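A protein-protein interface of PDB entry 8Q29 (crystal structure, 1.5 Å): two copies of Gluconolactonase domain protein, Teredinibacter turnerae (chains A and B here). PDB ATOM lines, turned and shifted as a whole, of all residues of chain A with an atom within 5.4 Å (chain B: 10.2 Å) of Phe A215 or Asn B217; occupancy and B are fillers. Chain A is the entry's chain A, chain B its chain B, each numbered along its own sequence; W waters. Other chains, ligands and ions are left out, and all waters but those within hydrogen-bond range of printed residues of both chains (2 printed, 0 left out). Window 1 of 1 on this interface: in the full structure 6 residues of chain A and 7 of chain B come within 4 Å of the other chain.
Trp A29 touches its own counterpart, Trp B29. Asn A99 touches Asn B217, and with the chains exchanged Asn A217 touches Asn B99. Phe A215 touches Asn B217, and with the chains exchanged Asn A217 touches Phe B215. Positions printed for both chains: 29, 99, 100, 101, 102, 213, 214, 215, 216 and 217. Of the 5 pairs that touch across the chains among the printed residues, 5 have their exchanged pair printed and touching as well.
Of the printed residues of chain B, Trp A29 touches Trp B29. His A100 touches none of the printed residues of chain B. No residue of chain B comes within 4 Å of Ser A214. Of the printed residues of chain B, Phe A215 touches Asn B217 (2.9 Å). Of the printed residues of chain A, Trp B29 touches Trp A29. Gly B63 touches none of the printed residues of chain A. Of the printed residues of chain A, Phe B215 touches Asn A217 (2.9 Å). Printed residues of chain A within 4 Å of Asn B217: Asn A99 (3.8 Å) and Phe A215 (2.9 Å). The nearest printed residue of chain B that does not touch Phe A215 is Ala B64 (5.4 Å). The nearest printed residue of chain A that does not touch Asn B217 is Asn A217 (4.5 Å). The nearest printed residue of chain A that does not touch Asn B99 is Ser A216 (8.0 Å).
The backbone carbonyl oxygen of Phe B215 lies within hydrogen-bond range of the side-chain amide nitrogen of Asn B99. O of His B100 sits at hydrogen-bond distance from N of Phe B215 (2.8 Å). The side-chain hydroxyl (OG) of Ser B214 lies within hydrogen-bond range of the backbone NH (N) of Asn B217 (3.4 Å). The backbone NH (N) of Asn A217 sits at hydrogen-bond distance from the side-chain hydroxyl (OG) of Ser A214 (3.4 Å). The side-chain amide nitrogen (ND2) of Asn A99 sits at hydrogen-bond distance from the backbone carbonyl oxygen (O) of Phe A215 (3.0 Å). OG of Ser A216 is in hydrogen-bond range of N of Asn A99, 2.9 Å away.
Among the printed residues, merely in contact across the chains: Trp A29 with Trp B29 (3.3 Å), Asn A99 with Asn B217 (3.8 Å) and Asn A217 with Asn B99 (3.8 Å).
Water W2 bridges the side-chain amide oxygen (OD1) of Asn A217 and the side-chain amide nitrogen (ND2) of Asn B99. Water W1 bridges the backbone carbonyl oxygen of Trp B29 (2.7 Å) and the backbone carbonyl oxygen of Trp A29 (2.9 Å).
Printed residues of chain A that touch a printed residue of chain B: Trp A29, Asn A99, Phe A215 and Asn A217.
The backbone carbonyl oxygen of Phe B215 lies within hydrogen-bond range of the side-chain amide nitrogen of Asn A217 (2.9 Å). The backbone carbonyl oxygen (O) of Phe A215 sits at hydrogen-bond distance from the side-chain amide nitrogen (ND2) of Asn B217 (2.9 Å).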
ATOM      1  N   TRP A  29     -13.936  29.141  -1.439  1.00  0.00           N
ATOM      2  CA  TRP A  29     -15.243  28.544  -1.219  1.00  0.00           C
ATOM      3  C   TRP A  29     -15.696  28.520   0.238  1.00  0.00           C
ATOM      4  O   TRP A  29     -16.666  27.848   0.563  1.00  0.00           O
ATOM      5  CB  TRP A  29     -15.311  27.151  -1.804  1.00  0.00           C
ATOM      6  CG  TRP A  29     -14.986  27.034  -3.255  1.00  0.00           C
ATOM      7  CD1 TRP A  29     -13.810  26.632  -3.784  1.00  0.00           C
ATOM      8  CD2 TRP A  29     -15.879  27.211  -4.351  1.00  0.00           C
ATOM      9  NE1 TRP A  29     -13.876  26.564  -5.130  1.00  0.00           N
ATOM     10  CE2 TRP A  29     -15.148  26.887  -5.510  1.00  0.00           C
ATOM     11  CE3 TRP A  29     -17.235  27.588  -4.476  1.00  0.00           C
ATOM     12  CZ2 TRP A  29     -15.696  26.936  -6.788  1.00  0.00           C
ATOM     13  CZ3 TRP A  29     -17.777  27.598  -5.746  1.00  0.00           C
ATOM     14  CH2 TRP A  29     -17.029  27.281  -6.872  1.00  0.00           C
ATOM     15  N   ASN A  99     -16.455  29.347 -20.425  1.00  0.00           N
ATOM     16  CA  ASN A  99     -17.616  28.804 -19.767  1.00  0.00           C
ATOM     17  C   ASN A  99     -18.446  29.937 -19.129  1.00  0.00           C
ATOM     18  O   ASN A  99     -19.465  30.331 -19.692  1.00  0.00           O
ATOM     19  CB  ASN A  99     -17.202  27.678 -18.788  1.00  0.00           C
ATOM     20  CG  ASN A  99     -18.376  26.978 -18.151  1.00  0.00           C
ATOM     21  OD1 ASN A  99     -19.464  26.955 -18.742  1.00  0.00           O
ATOM     22  ND2 ASN A  99     -18.165  26.366 -16.998  1.00  0.00           N
ATOM     23  N   HIS A 100     -17.984  30.469 -18.006  1.00  0.00           N
ATOM     24  CA  HIS A 100     -18.468  31.736 -17.453  1.00  0.00           C
ATOM     25  C   HIS A 100     -17.527  32.176 -16.328  1.00  0.00           C
ATOM     26  O   HIS A 100     -16.881  31.338 -15.683  1.00  0.00           O
ATOM     27  CB  HIS A 100     -19.910  31.610 -16.955  1.00  0.00           C
ATOM     28  CG  HIS A 100     -20.226  30.508 -15.977  1.00  0.00           C
ATOM     29  ND1 HIS A 100     -20.242  30.684 -14.608  1.00  0.00           N
ATOM     30  CD2 HIS A 100     -20.516  29.168 -16.192  1.00  0.00           C
ATOM     31  CE1 HIS A 100     -20.570  29.507 -14.021  1.00  0.00           C
ATOM     32  NE2 HIS A 100     -20.697  28.566 -14.971  1.00  0.00           N
ATOM     33  N   GLU A 101     -17.514  33.496 -16.068  1.00  0.00           N
ATOM     34  CA  GLU A 101     -16.680  34.078 -15.032  1.00  0.00           C
ATOM     35  C   GLU A 101     -17.371  35.339 -14.510  1.00  0.00           C
ATOM     36  O   GLU A 101     -18.082  35.955 -15.292  1.00  0.00           O
ATOM     37  CB  GLU A 101     -15.307  34.495 -15.606  1.00  0.00           C
ATOM     38  CG  GLU A 101     -14.629  33.425 -16.390  1.00  0.00           C
ATOM     39  CD  GLU A 101     -13.254  33.829 -16.844  1.00  0.00           C
ATOM     40  OE1 GLU A 101     -13.168  34.885 -17.570  1.00  0.00           O
ATOM     41  OE2 GLU A 101     -12.266  33.074 -16.491  1.00  0.00           O
ATOM     42  N   HIS A 102     -17.166  35.696 -13.248  1.00  0.00           N
ATOM     43  CA  HIS A 102     -17.818  36.891 -12.754  1.00  0.00           C
ATOM     44  C   HIS A 102     -17.024  37.672 -11.737  1.00  0.00           C
ATOM     45  O   HIS A 102     -16.187  37.162 -10.987  1.00  0.00           O
ATOM     46  CB  HIS A 102     -19.208  36.537 -12.237  1.00  0.00           C
ATOM     47  CG  HIS A 102     -19.189  35.649 -11.049  1.00  0.00           C
ATOM     48  ND1 HIS A 102     -19.179  34.237 -11.116  1.00  0.00           N
ATOM     49  CD2 HIS A 102     -19.267  35.983  -9.763  1.00  0.00           C
ATOM     50  CE1 HIS A 102     -19.235  33.777  -9.891  1.00  0.00           C
ATOM     51  NE2 HIS A 102     -19.289  34.794  -9.022  1.00  0.00           N
ATOM     52  N   ARG A 118     -24.675  36.308 -10.805  1.00  0.00           N
ATOM     53  CA  ARG A 118     -23.257  36.431 -11.118  1.00  0.00           C
ATOM     54  C   ARG A 118     -23.095  37.232 -12.419  1.00  0.00           C
ATOM     55  O   ARG A 118     -23.468  36.733 -13.480  1.00  0.00           O
ATOM     56  CB  ARG A 118     -22.649  35.049 -11.340  1.00  0.00           C
ATOM     57  CG  ARG A 118     -22.693  34.159 -10.109  1.00  0.00           C
ATOM     58  CD  ARG A 118     -22.442  32.728 -10.639  1.00  0.00           C
ATOM     59  NE  ARG A 118     -22.253  31.839  -9.541  1.00  0.00           N
ATOM     60  CZ  ARG A 118     -22.052  30.531  -9.651  1.00  0.00           C
ATOM     61  NH1 ARG A 118     -22.079  29.951 -10.827  1.00  0.00           N
ATOM     62  NH2 ARG A 118     -21.831  29.830  -8.562  1.00  0.00           N
ATOM     63  N   HIS A 213     -14.097  35.217  -9.762  1.00  0.00           N
ATOM     64  CA  HIS A 213     -14.514  33.820  -9.707  1.00  0.00           C
ATOM     65  C   HIS A 213     -14.655  33.326 -11.142  1.00  0.00           C
ATOM     66  O   HIS A 213     -15.556  33.771 -11.882  1.00  0.00           O
ATOM     67  CB  HIS A 213     -15.819  33.688  -8.878  1.00  0.00           C
ATOM     68  CG  HIS A 213     -16.133  32.289  -8.466  1.00  0.00           C
ATOM     69  ND1 HIS A 213     -17.239  31.998  -7.686  1.00  0.00           N
ATOM     70  CD2 HIS A 213     -15.491  31.112  -8.697  1.00  0.00           C
ATOM     71  CE1 HIS A 213     -17.233  30.688  -7.420  1.00  0.00           C
ATOM     72  NE2 HIS A 213     -16.172  30.147  -8.018  1.00  0.00           N
ATOM     73  N   SER A 214     -13.806  32.344 -11.541  1.00  0.00           N
ATOM     74  CA  SER A 214     -13.849  31.810 -12.899  1.00  0.00           C
ATOM     75  C   SER A 214     -14.396  30.378 -12.829  1.00  0.00           C
ATOM     76  O   SER A 214     -13.975  29.565 -11.974  1.00  0.00           O
ATOM     77  CB  SER A 214     -12.455  31.805 -13.480  1.00  0.00           C
ATOM     78  OG  SER A 214     -12.412  31.252 -14.773  1.00  0.00           O
ATOM     79  N   PHE A 215     -15.315  30.065 -13.731  1.00  0.00           N
ATOM     80  CA  PHE A 215     -15.724  28.700 -14.001  1.00  0.00           C
ATOM     81  C   PHE A 215     -15.113  28.235 -15.321  1.00  0.00           C
ATOM     82  O   PHE A 215     -15.552  27.211 -15.869  1.00  0.00           O
ATOM     83  CB  PHE A 215     -17.251  28.564 -13.934  1.00  0.00           C
ATOM     84  CG  PHE A 215     -17.784  28.652 -12.550  1.00  0.00           C
ATOM     85  CD1 PHE A 215     -17.959  29.886 -11.951  1.00  0.00           C
ATOM     86  CD2 PHE A 215     -18.182  27.537 -11.835  1.00  0.00           C
ATOM     87  CE1 PHE A 215     -18.430  30.015 -10.660  1.00  0.00           C
ATOM     88  CE2 PHE A 215     -18.693  27.678 -10.565  1.00  0.00           C
ATOM     89  CZ  PHE A 215     -18.766  28.898  -9.941  1.00  0.00           C
ATOM     90  N   SER A 216     -14.039  28.934 -15.734  1.00  0.00           N
ATOM     91  CA  SER A 216     -13.346  28.671 -16.988  1.00  0.00           C
ATOM     92  C   SER A 216     -11.882  28.327 -16.701  1.00  0.00           C
ATOM     93  O   SER A 216     -11.041  28.316 -17.599  1.00  0.00           O
ATOM     94  CB  SER A 216     -13.455  29.832 -17.929  1.00  0.00           C
ATOM     95  OG  SER A 216     -14.836  30.184 -18.228  1.00  0.00           O
ATOM     96  N   ASN A 217     -11.576  27.994 -15.443  1.00  0.00           N
ATOM     97  CA  ASN A 217     -10.237  27.613 -15.027  1.00  0.00           C
ATOM     98  C   ASN A 217      -9.223  28.705 -15.368  1.00  0.00           C
ATOM     99  O   ASN A 217      -8.084  28.400 -15.707  1.00  0.00           O
ATOM    100  CB  ASN A 217      -9.835  26.220 -15.566  1.00  0.00           C
ATOM    101  CG  ASN A 217     -10.319  25.031 -14.739  1.00  0.00           C
ATOM    102  OD1 ASN A 217     -10.424  25.101 -13.512  1.00  0.00           O
ATOM    103  ND2 ASN A 217     -10.608  23.904 -15.383  1.00  0.00           N
ATOM    104  N   GLY B  28     -21.132  20.330  -2.781  1.00  0.00           N
ATOM    105  CA  GLY B  28     -21.239  21.735  -3.171  1.00  0.00           C
ATOM    106  C   GLY B  28     -20.317  22.673  -2.418  1.00  0.00           C
ATOM    107  O   GLY B  28     -20.681  23.830  -2.177  1.00  0.00           O
ATOM    108  N   TRP B  29     -19.151  22.157  -2.031  1.00  0.00           N
ATOM    109  CA  TRP B  29     -18.073  22.870  -1.330  1.00  0.00           C
ATOM    110  C   TRP B  29     -18.394  23.153   0.138  1.00  0.00           C
ATOM    111  O   TRP B  29     -17.723  23.963   0.790  1.00  0.00           O
ATOM    112  CB  TRP B  29     -17.658  24.173  -2.012  1.00  0.00           C
ATOM    113  CG  TRP B  29     -17.242  23.992  -3.446  1.00  0.00           C
ATOM    114  CD1 TRP B  29     -17.984  24.212  -4.553  1.00  0.00           C
ATOM    115  CD2 TRP B  29     -15.949  23.599  -3.900  1.00  0.00           C
ATOM    116  NE1 TRP B  29     -17.258  23.992  -5.691  1.00  0.00           N
ATOM    117  CE2 TRP B  29     -15.979  23.669  -5.316  1.00  0.00           C
ATOM    118  CE3 TRP B  29     -14.742  23.302  -3.258  1.00  0.00           C
ATOM    119  CZ2 TRP B  29     -14.885  23.367  -6.098  1.00  0.00           C
ATOM    120  CZ3 TRP B  29     -13.649  23.046  -4.057  1.00  0.00           C
ATOM    121  CH2 TRP B  29     -13.697  23.124  -5.429  1.00  0.00           C
ATOM    122  N   GLY B  62     -22.254  14.734  -9.247  1.00  0.00           N
ATOM    123  CA  GLY B  62     -21.593  16.027  -9.124  1.00  0.00           C
ATOM    124  C   GLY B  62     -20.757  16.374 -10.344  1.00  0.00           C
ATOM    125  O   GLY B  62     -20.956  15.839 -11.417  1.00  0.00           O
ATOM    126  N   GLY B  63     -19.795  17.250 -10.168  1.00  0.00           N
ATOM    127  CA  GLY B  63     -19.020  17.727 -11.264  1.00  0.00           C
ATOM    128  C   GLY B  63     -17.897  18.631 -10.777  1.00  0.00           C
ATOM    129  O   GLY B  63     -17.176  18.328  -9.847  1.00  0.00           O
ATOM    130  N   ALA B  64     -17.944  19.872 -11.276  1.00  0.00           N
ATOM    131  CA  ALA B  64     -17.133  20.927 -10.703  1.00  0.00           C
ATOM    132  C   ALA B  64     -17.473  21.151  -9.238  1.00  0.00           C
ATOM    133  O   ALA B  64     -16.599  21.510  -8.437  1.00  0.00           O
ATOM    134  CB  ALA B  64     -17.331  22.209 -11.468  1.00  0.00           C
ATOM    135  N   ALA B  65     -18.755  20.965  -8.929  1.00  0.00           N
ATOM    136  CA  ALA B  65     -19.187  20.986  -7.543  1.00  0.00           C
ATOM    137  C   ALA B  65     -18.973  19.585  -7.000  1.00  0.00           C
ATOM    138  O   ALA B  65     -19.475  18.617  -7.562  1.00  0.00           O
ATOM    139  CB  ALA B  65     -20.640  21.365  -7.439  1.00  0.00           C
ATOM    140  N   PRO B  66     -18.229  19.430  -5.885  1.00  0.00           N
ATOM    141  CA  PRO B  66     -17.954  18.084  -5.397  1.00  0.00           C
ATOM    142  C   PRO B  66     -19.184  17.440  -4.787  1.00  0.00           C
ATOM    143  O   PRO B  66     -20.051  18.078  -4.182  1.00  0.00           O
ATOM    144  CB  PRO B  66     -16.877  18.310  -4.354  1.00  0.00           C
ATOM    145  CG  PRO B  66     -17.204  19.679  -3.803  1.00  0.00           C
ATOM    146  CD  PRO B  66     -17.586  20.439  -5.056  1.00  0.00           C
ATOM    147  N   LYS B  90     -17.755   8.125 -16.571  1.00  0.00           N
ATOM    148  CA  LYS B  90     -16.701   8.500 -17.483  1.00  0.00           C
ATOM    149  C   LYS B  90     -15.419   7.832 -16.989  1.00  0.00           C
ATOM    150  O   LYS B  90     -15.365   7.308 -15.873  1.00  0.00           O
ATOM    151  CB  LYS B  90     -16.512  10.027 -17.602  1.00  0.00           C
ATOM    152  CG  LYS B  90     -15.936  10.692 -16.355  1.00  0.00           C
ATOM    153  CD  LYS B  90     -15.656  12.182 -16.512  1.00  0.00           C
ATOM    154  CE  LYS B  90     -14.600  12.466 -17.547  1.00  0.00           C
ATOM    155  NZ  LYS B  90     -13.263  12.041 -17.096  1.00  0.00           N
ATOM    156  N   GLU B  95      -6.533  10.573 -20.994  1.00  0.00           N
ATOM    157  CA  GLU B  95      -7.580  11.511 -21.373  1.00  0.00           C
ATOM    158  C   GLU B  95      -6.997  12.894 -21.760  1.00  0.00           C
ATOM    159  O   GLU B  95      -6.588  13.715 -20.934  1.00  0.00           O
ATOM    160  CB  GLU B  95      -8.631  11.642 -20.281  1.00  0.00           C
ATOM    161  CG  GLU B  95      -9.856  12.397 -20.773  1.00  0.00           C
ATOM    162  CD  GLU B  95     -11.094  12.269 -19.903  1.00  0.00           C
ATOM    163  OE1 GLU B  95     -11.098  12.599 -18.751  1.00  0.00           O
ATOM    164  OE2 GLU B  95     -12.126  11.945 -20.470  1.00  0.00           O
ATOM    165  N   GLY B  97      -6.854  16.685 -22.681  1.00  0.00           N
ATOM    166  CA  GLY B  97      -7.552  17.916 -22.253  1.00  0.00           C
ATOM    167  C   GLY B  97      -7.885  17.996 -20.771  1.00  0.00           C
ATOM    168  O   GLY B  97      -8.384  19.015 -20.331  1.00  0.00           O
ATOM    169  N   ASP B  98      -7.672  16.910 -20.016  1.00  0.00           N
ATOM    170  CA  ASP B  98      -8.035  16.943 -18.597  1.00  0.00           C
ATOM    171  C   ASP B  98      -7.126  17.907 -17.808  1.00  0.00           C
ATOM    172  O   ASP B  98      -5.907  18.033 -18.043  1.00  0.00           O
ATOM    173  CB  ASP B  98      -7.860  15.523 -18.050  1.00  0.00           C
ATOM    174  CG  ASP B  98      -8.117  15.460 -16.558  1.00  0.00           C
ATOM    175  OD1 ASP B  98      -9.294  15.723 -16.182  1.00  0.00           O
ATOM    176  OD2 ASP B  98      -7.141  15.151 -15.804  1.00  0.00           O
ATOM    177  N   ASN B  99      -7.728  18.528 -16.790  1.00  0.00           N
ATOM    178  CA  ASN B  99      -7.030  19.292 -15.770  1.00  0.00           C
ATOM    179  C   ASN B  99      -6.671  18.360 -14.594  1.00  0.00           C
ATOM    180  O   ASN B  99      -5.513  17.991 -14.406  1.00  0.00           O
ATOM    181  CB  ASN B  99      -7.797  20.556 -15.395  1.00  0.00           C
ATOM    182  CG  ASN B  99      -7.048  21.411 -14.395  1.00  0.00           C
ATOM    183  OD1 ASN B  99      -5.805  21.385 -14.318  1.00  0.00           O
ATOM    184  ND2 ASN B  99      -7.767  22.187 -13.609  1.00  0.00           N
ATOM    185  N   HIS B 100      -7.659  18.008 -13.807  1.00  0.00           N
ATOM    186  CA  HIS B 100      -7.542  16.911 -12.850  1.00  0.00           C
ATOM    187  C   HIS B 100      -8.931  16.612 -12.284  1.00  0.00           C
ATOM    188  O   HIS B 100      -9.801  17.469 -12.246  1.00  0.00           O
ATOM    189  CB  HIS B 100      -6.560  17.201 -11.713  1.00  0.00           C
ATOM    190  CG  HIS B 100      -6.737  18.489 -10.980  1.00  0.00           C
ATOM    191  ND1 HIS B 100      -7.359  18.557  -9.733  1.00  0.00           N
ATOM    192  CD2 HIS B 100      -6.337  19.745 -11.276  1.00  0.00           C
ATOM    193  CE1 HIS B 100      -7.291  19.828  -9.315  1.00  0.00           C
ATOM    194  NE2 HIS B 100      -6.697  20.562 -10.227  1.00  0.00           N
ATOM    195  N   GLU B 101      -9.125  15.365 -11.814  1.00  0.00           N
ATOM    196  CA  GLU B 101     -10.357  14.918 -11.241  1.00  0.00           C
ATOM    197  C   GLU B 101     -10.067  13.796 -10.246  1.00  0.00           C
ATOM    198  O   GLU B 101      -9.100  13.072 -10.459  1.00  0.00           O
ATOM    199  CB  GLU B 101     -11.335  14.341 -12.289  1.00  0.00           C
ATOM    200  CG  GLU B 101     -11.541  15.227 -13.514  1.00  0.00           C
ATOM    201  CD  GLU B 101     -12.442  14.631 -14.549  1.00  0.00           C
ATOM    202  OE1 GLU B 101     -12.176  13.465 -14.995  1.00  0.00           O
ATOM    203  OE2 GLU B 101     -13.416  15.318 -14.910  1.00  0.00           O
ATOM    204  N   HIS B 102     -10.873  13.697  -9.199  1.00  0.00           N
ATOM    205  CA  HIS B 102     -10.579  12.667  -8.189  1.00  0.00           C
ATOM    206  C   HIS B 102     -11.793  12.033  -7.557  1.00  0.00           C
ATOM    207  O   HIS B 102     -12.878  12.605  -7.463  1.00  0.00           O
ATOM    208  CB  HIS B 102      -9.582  13.188  -7.138  1.00  0.00           C
ATOM    209  CG  HIS B 102     -10.161  14.261  -6.315  1.00  0.00           C
ATOM    210  ND1 HIS B 102     -10.092  15.580  -6.681  1.00  0.00           N
ATOM    211  CD2 HIS B 102     -10.712  14.227  -5.060  1.00  0.00           C
ATOM    212  CE1 HIS B 102     -10.683  16.298  -5.714  1.00  0.00           C
ATOM    213  NE2 HIS B 102     -11.065  15.500  -4.715  1.00  0.00           N
ATOM    214  N   GLN B 121      -7.273  11.276 -11.496  1.00  0.00           N
ATOM    215  CA  GLN B 121      -6.317  11.590 -12.543  1.00  0.00           C
ATOM    216  C   GLN B 121      -5.855  13.052 -12.409  1.00  0.00           C
ATOM    217  O   GLN B 121      -6.536  13.890 -11.820  1.00  0.00           O
ATOM    218  CB  GLN B 121      -6.854  11.359 -13.978  1.00  0.00           C
ATOM    219  CG  GLN B 121      -7.996  12.249 -14.385  1.00  0.00           C
ATOM    220  CD  GLN B 121      -8.481  11.994 -15.801  1.00  0.00           C
ATOM    221  OE1 GLN B 121      -7.758  11.394 -16.625  1.00  0.00           O
ATOM    222  NE2 GLN B 121      -9.683  12.432 -16.121  1.00  0.00           N
ATOM    223  N   TRP B 212     -17.090  12.206  -6.201  1.00  0.00           N
ATOM    224  CA  TRP B 212     -16.682  12.764  -7.467  1.00  0.00           C
ATOM    225  C   TRP B 212     -16.378  14.231  -7.331  1.00  0.00           C
ATOM    226  O   TRP B 212     -17.161  14.965  -6.744  1.00  0.00           O
ATOM    227  CB  TRP B 212     -17.761  12.603  -8.555  1.00  0.00           C
ATOM    228  CG  TRP B 212     -17.338  13.134  -9.902  1.00  0.00           C
ATOM    229  CD1 TRP B 212     -17.802  14.251 -10.549  1.00  0.00           C
ATOM    230  CD2 TRP B 212     -16.266  12.634 -10.725  1.00  0.00           C
ATOM    231  NE1 TRP B 212     -17.101  14.433 -11.716  1.00  0.00           N
ATOM    232  CE2 TRP B 212     -16.137  13.478 -11.846  1.00  0.00           C
ATOM    233  CE3 TRP B 212     -15.407  11.541 -10.629  1.00  0.00           C
ATOM    234  CZ2 TRP B 212     -15.216  13.233 -12.868  1.00  0.00           C
ATOM    235  CZ3 TRP B 212     -14.475  11.308 -11.624  1.00  0.00           C
ATOM    236  CH2 TRP B 212     -14.400  12.136 -12.747  1.00  0.00           C
ATOM    237  N   HIS B 213     -15.231  14.631  -7.829  1.00  0.00           N
ATOM    238  CA  HIS B 213     -14.831  16.028  -7.814  1.00  0.00           C
ATOM    239  C   HIS B 213     -13.987  16.274  -9.044  1.00  0.00           C
ATOM    240  O   HIS B 213     -12.856  15.786  -9.124  1.00  0.00           O
ATOM    241  CB  HIS B 213     -14.107  16.385  -6.512  1.00  0.00           C
ATOM    242  CG  HIS B 213     -13.963  17.859  -6.242  1.00  0.00           C
ATOM    243  ND1 HIS B 213     -13.337  18.365  -5.127  1.00  0.00           N
ATOM    244  CD2 HIS B 213     -14.375  18.905  -6.991  1.00  0.00           C
ATOM    245  CE1 HIS B 213     -13.382  19.690  -5.211  1.00  0.00           C
ATOM    246  NE2 HIS B 213     -14.044  20.044  -6.320  1.00  0.00           N
ATOM    247  N   SER B 214     -14.524  17.100  -9.977  1.00  0.00           N
ATOM    248  CA  SER B 214     -13.818  17.383 -11.219  1.00  0.00           C
ATOM    249  C   SER B 214     -13.305  18.828 -11.226  1.00  0.00           C
ATOM    250  O   SER B 214     -14.038  19.758 -10.848  1.00  0.00           O
ATOM    251  CB  SER B 214     -14.755  17.223 -12.417  1.00  0.00           C
ATOM    252  OG  SER B 214     -14.102  17.523 -13.663  1.00  0.00           O
ATOM    253  N   PHE B 215     -12.035  19.010 -11.609  1.00  0.00           N
ATOM    254  CA  PHE B 215     -11.516  20.317 -11.915  1.00  0.00           C
ATOM    255  C   PHE B 215     -11.354  20.490 -13.420  1.00  0.00           C
ATOM    256  O   PHE B 215     -10.650  21.384 -13.864  1.00  0.00           O
ATOM    257  CB  PHE B 215     -10.168  20.562 -11.179  1.00  0.00           C
ATOM    258  CG  PHE B 215     -10.348  20.682  -9.689  1.00  0.00           C
ATOM    259  CD1 PHE B 215     -10.560  19.592  -8.868  1.00  0.00           C
ATOM    260  CD2 PHE B 215     -10.353  21.934  -9.122  1.00  0.00           C
ATOM    261  CE1 PHE B 215     -10.742  19.753  -7.486  1.00  0.00           C
ATOM    262  CE2 PHE B 215     -10.505  22.107  -7.761  1.00  0.00           C
ATOM    263  CZ  PHE B 215     -10.722  21.013  -6.949  1.00  0.00           C
ATOM    264  N   SER B 216     -12.080  19.667 -14.159  1.00  0.00           N
ATOM    265  CA  SER B 216     -12.097  19.651 -15.616  1.00  0.00           C
ATOM    266  C   SER B 216     -13.490  19.958 -16.157  1.00  0.00           C
ATOM    267  O   SER B 216     -13.774  19.727 -17.338  1.00  0.00           O
ATOM    268  CB  SER B 216     -11.599  18.312 -16.077  1.00  0.00           C
ATOM    269  OG  SER B 216     -10.250  18.093 -15.673  1.00  0.00           O
ATOM    270  N   ASN B 217     -14.351  20.509 -15.301  1.00  0.00           N
ATOM    271  CA  ASN B 217     -15.701  20.888 -15.737  1.00  0.00           C
ATOM    272  C   ASN B 217     -16.471  19.686 -16.306  1.00  0.00           C
ATOM    273  O   ASN B 217     -17.308  19.840 -17.209  1.00  0.00           O
ATOM    274  CB  ASN B 217     -15.649  22.098 -16.682  1.00  0.00           C
ATOM    275  CG  ASN B 217     -15.605  23.405 -15.897  1.00  0.00           C
ATOM    276  OD1 ASN B 217     -16.254  23.546 -14.845  1.00  0.00           O
ATOM    277  ND2 ASN B 217     -14.931  24.393 -16.450  1.00  0.00           N
ATOM    278  N   ASN B 218     -16.254  18.456 -15.754  1.00  0.00           N
ATOM    279  CA  ASN B 218     -17.038  17.315 -16.179  1.00  0.00           C
ATOM    280  C   ASN B 218     -18.002  16.809 -15.100  1.00  0.00           C
ATOM    281  O   ASN B 218     -17.609  16.373 -13.996  1.00  0.00           O
ATOM    282  CB  ASN B 218     -16.171  16.135 -16.580  1.00  0.00           C
ATOM    283  CG  ASN B 218     -15.266  16.445 -17.764  1.00  0.00           C
ATOM    284  OD1 ASN B 218     -15.667  17.047 -18.761  1.00  0.00           O
ATOM    285  ND2 ASN B 218     -13.997  16.145 -17.608  1.00  0.00           N
ATOM    286  N   ASN B 219     -19.294  16.839 -15.451  1.00  0.00           N
ATOM    287  CA  ASN B 219     -20.279  16.195 -14.644  1.00  0.00           C
ATOM    288  C   ASN B 219     -20.117  14.675 -14.729  1.00  0.00           C
ATOM    289  O   ASN B 219     -19.768  14.147 -15.780  1.00  0.00           O
ATOM    290  CB  ASN B 219     -21.690  16.551 -15.102  1.00  0.00           C
ATOM    291  CG  ASN B 219     -22.021  18.006 -14.892  1.00  0.00           C
ATOM    292  OD1 ASN B 219     -21.537  18.645 -13.990  1.00  0.00           O
ATOM    293  ND2 ASN B 219     -22.979  18.469 -15.666  1.00  0.00           N
ATOM    294  N   ALA B 220     -20.364  13.988 -13.627  1.00  0.00           N
ATOM    295  CA  ALA B 220     -20.371  12.536 -13.608  1.00  0.00           C
ATOM    296  C   ALA B 220     -21.341  12.006 -12.568  1.00  0.00           C
ATOM    297  O   ALA B 220     -21.652  12.698 -11.586  1.00  0.00           O
ATOM    298  CB  ALA B 220     -18.963  12.001 -13.374  1.00  0.00           C
HETATM  299  O   HOH W   1     -17.618  26.050   2.565  1.00  0.00           O
HETATM  300  O   HOH W   2      -8.907  24.515 -11.321  1.00  0.00           O
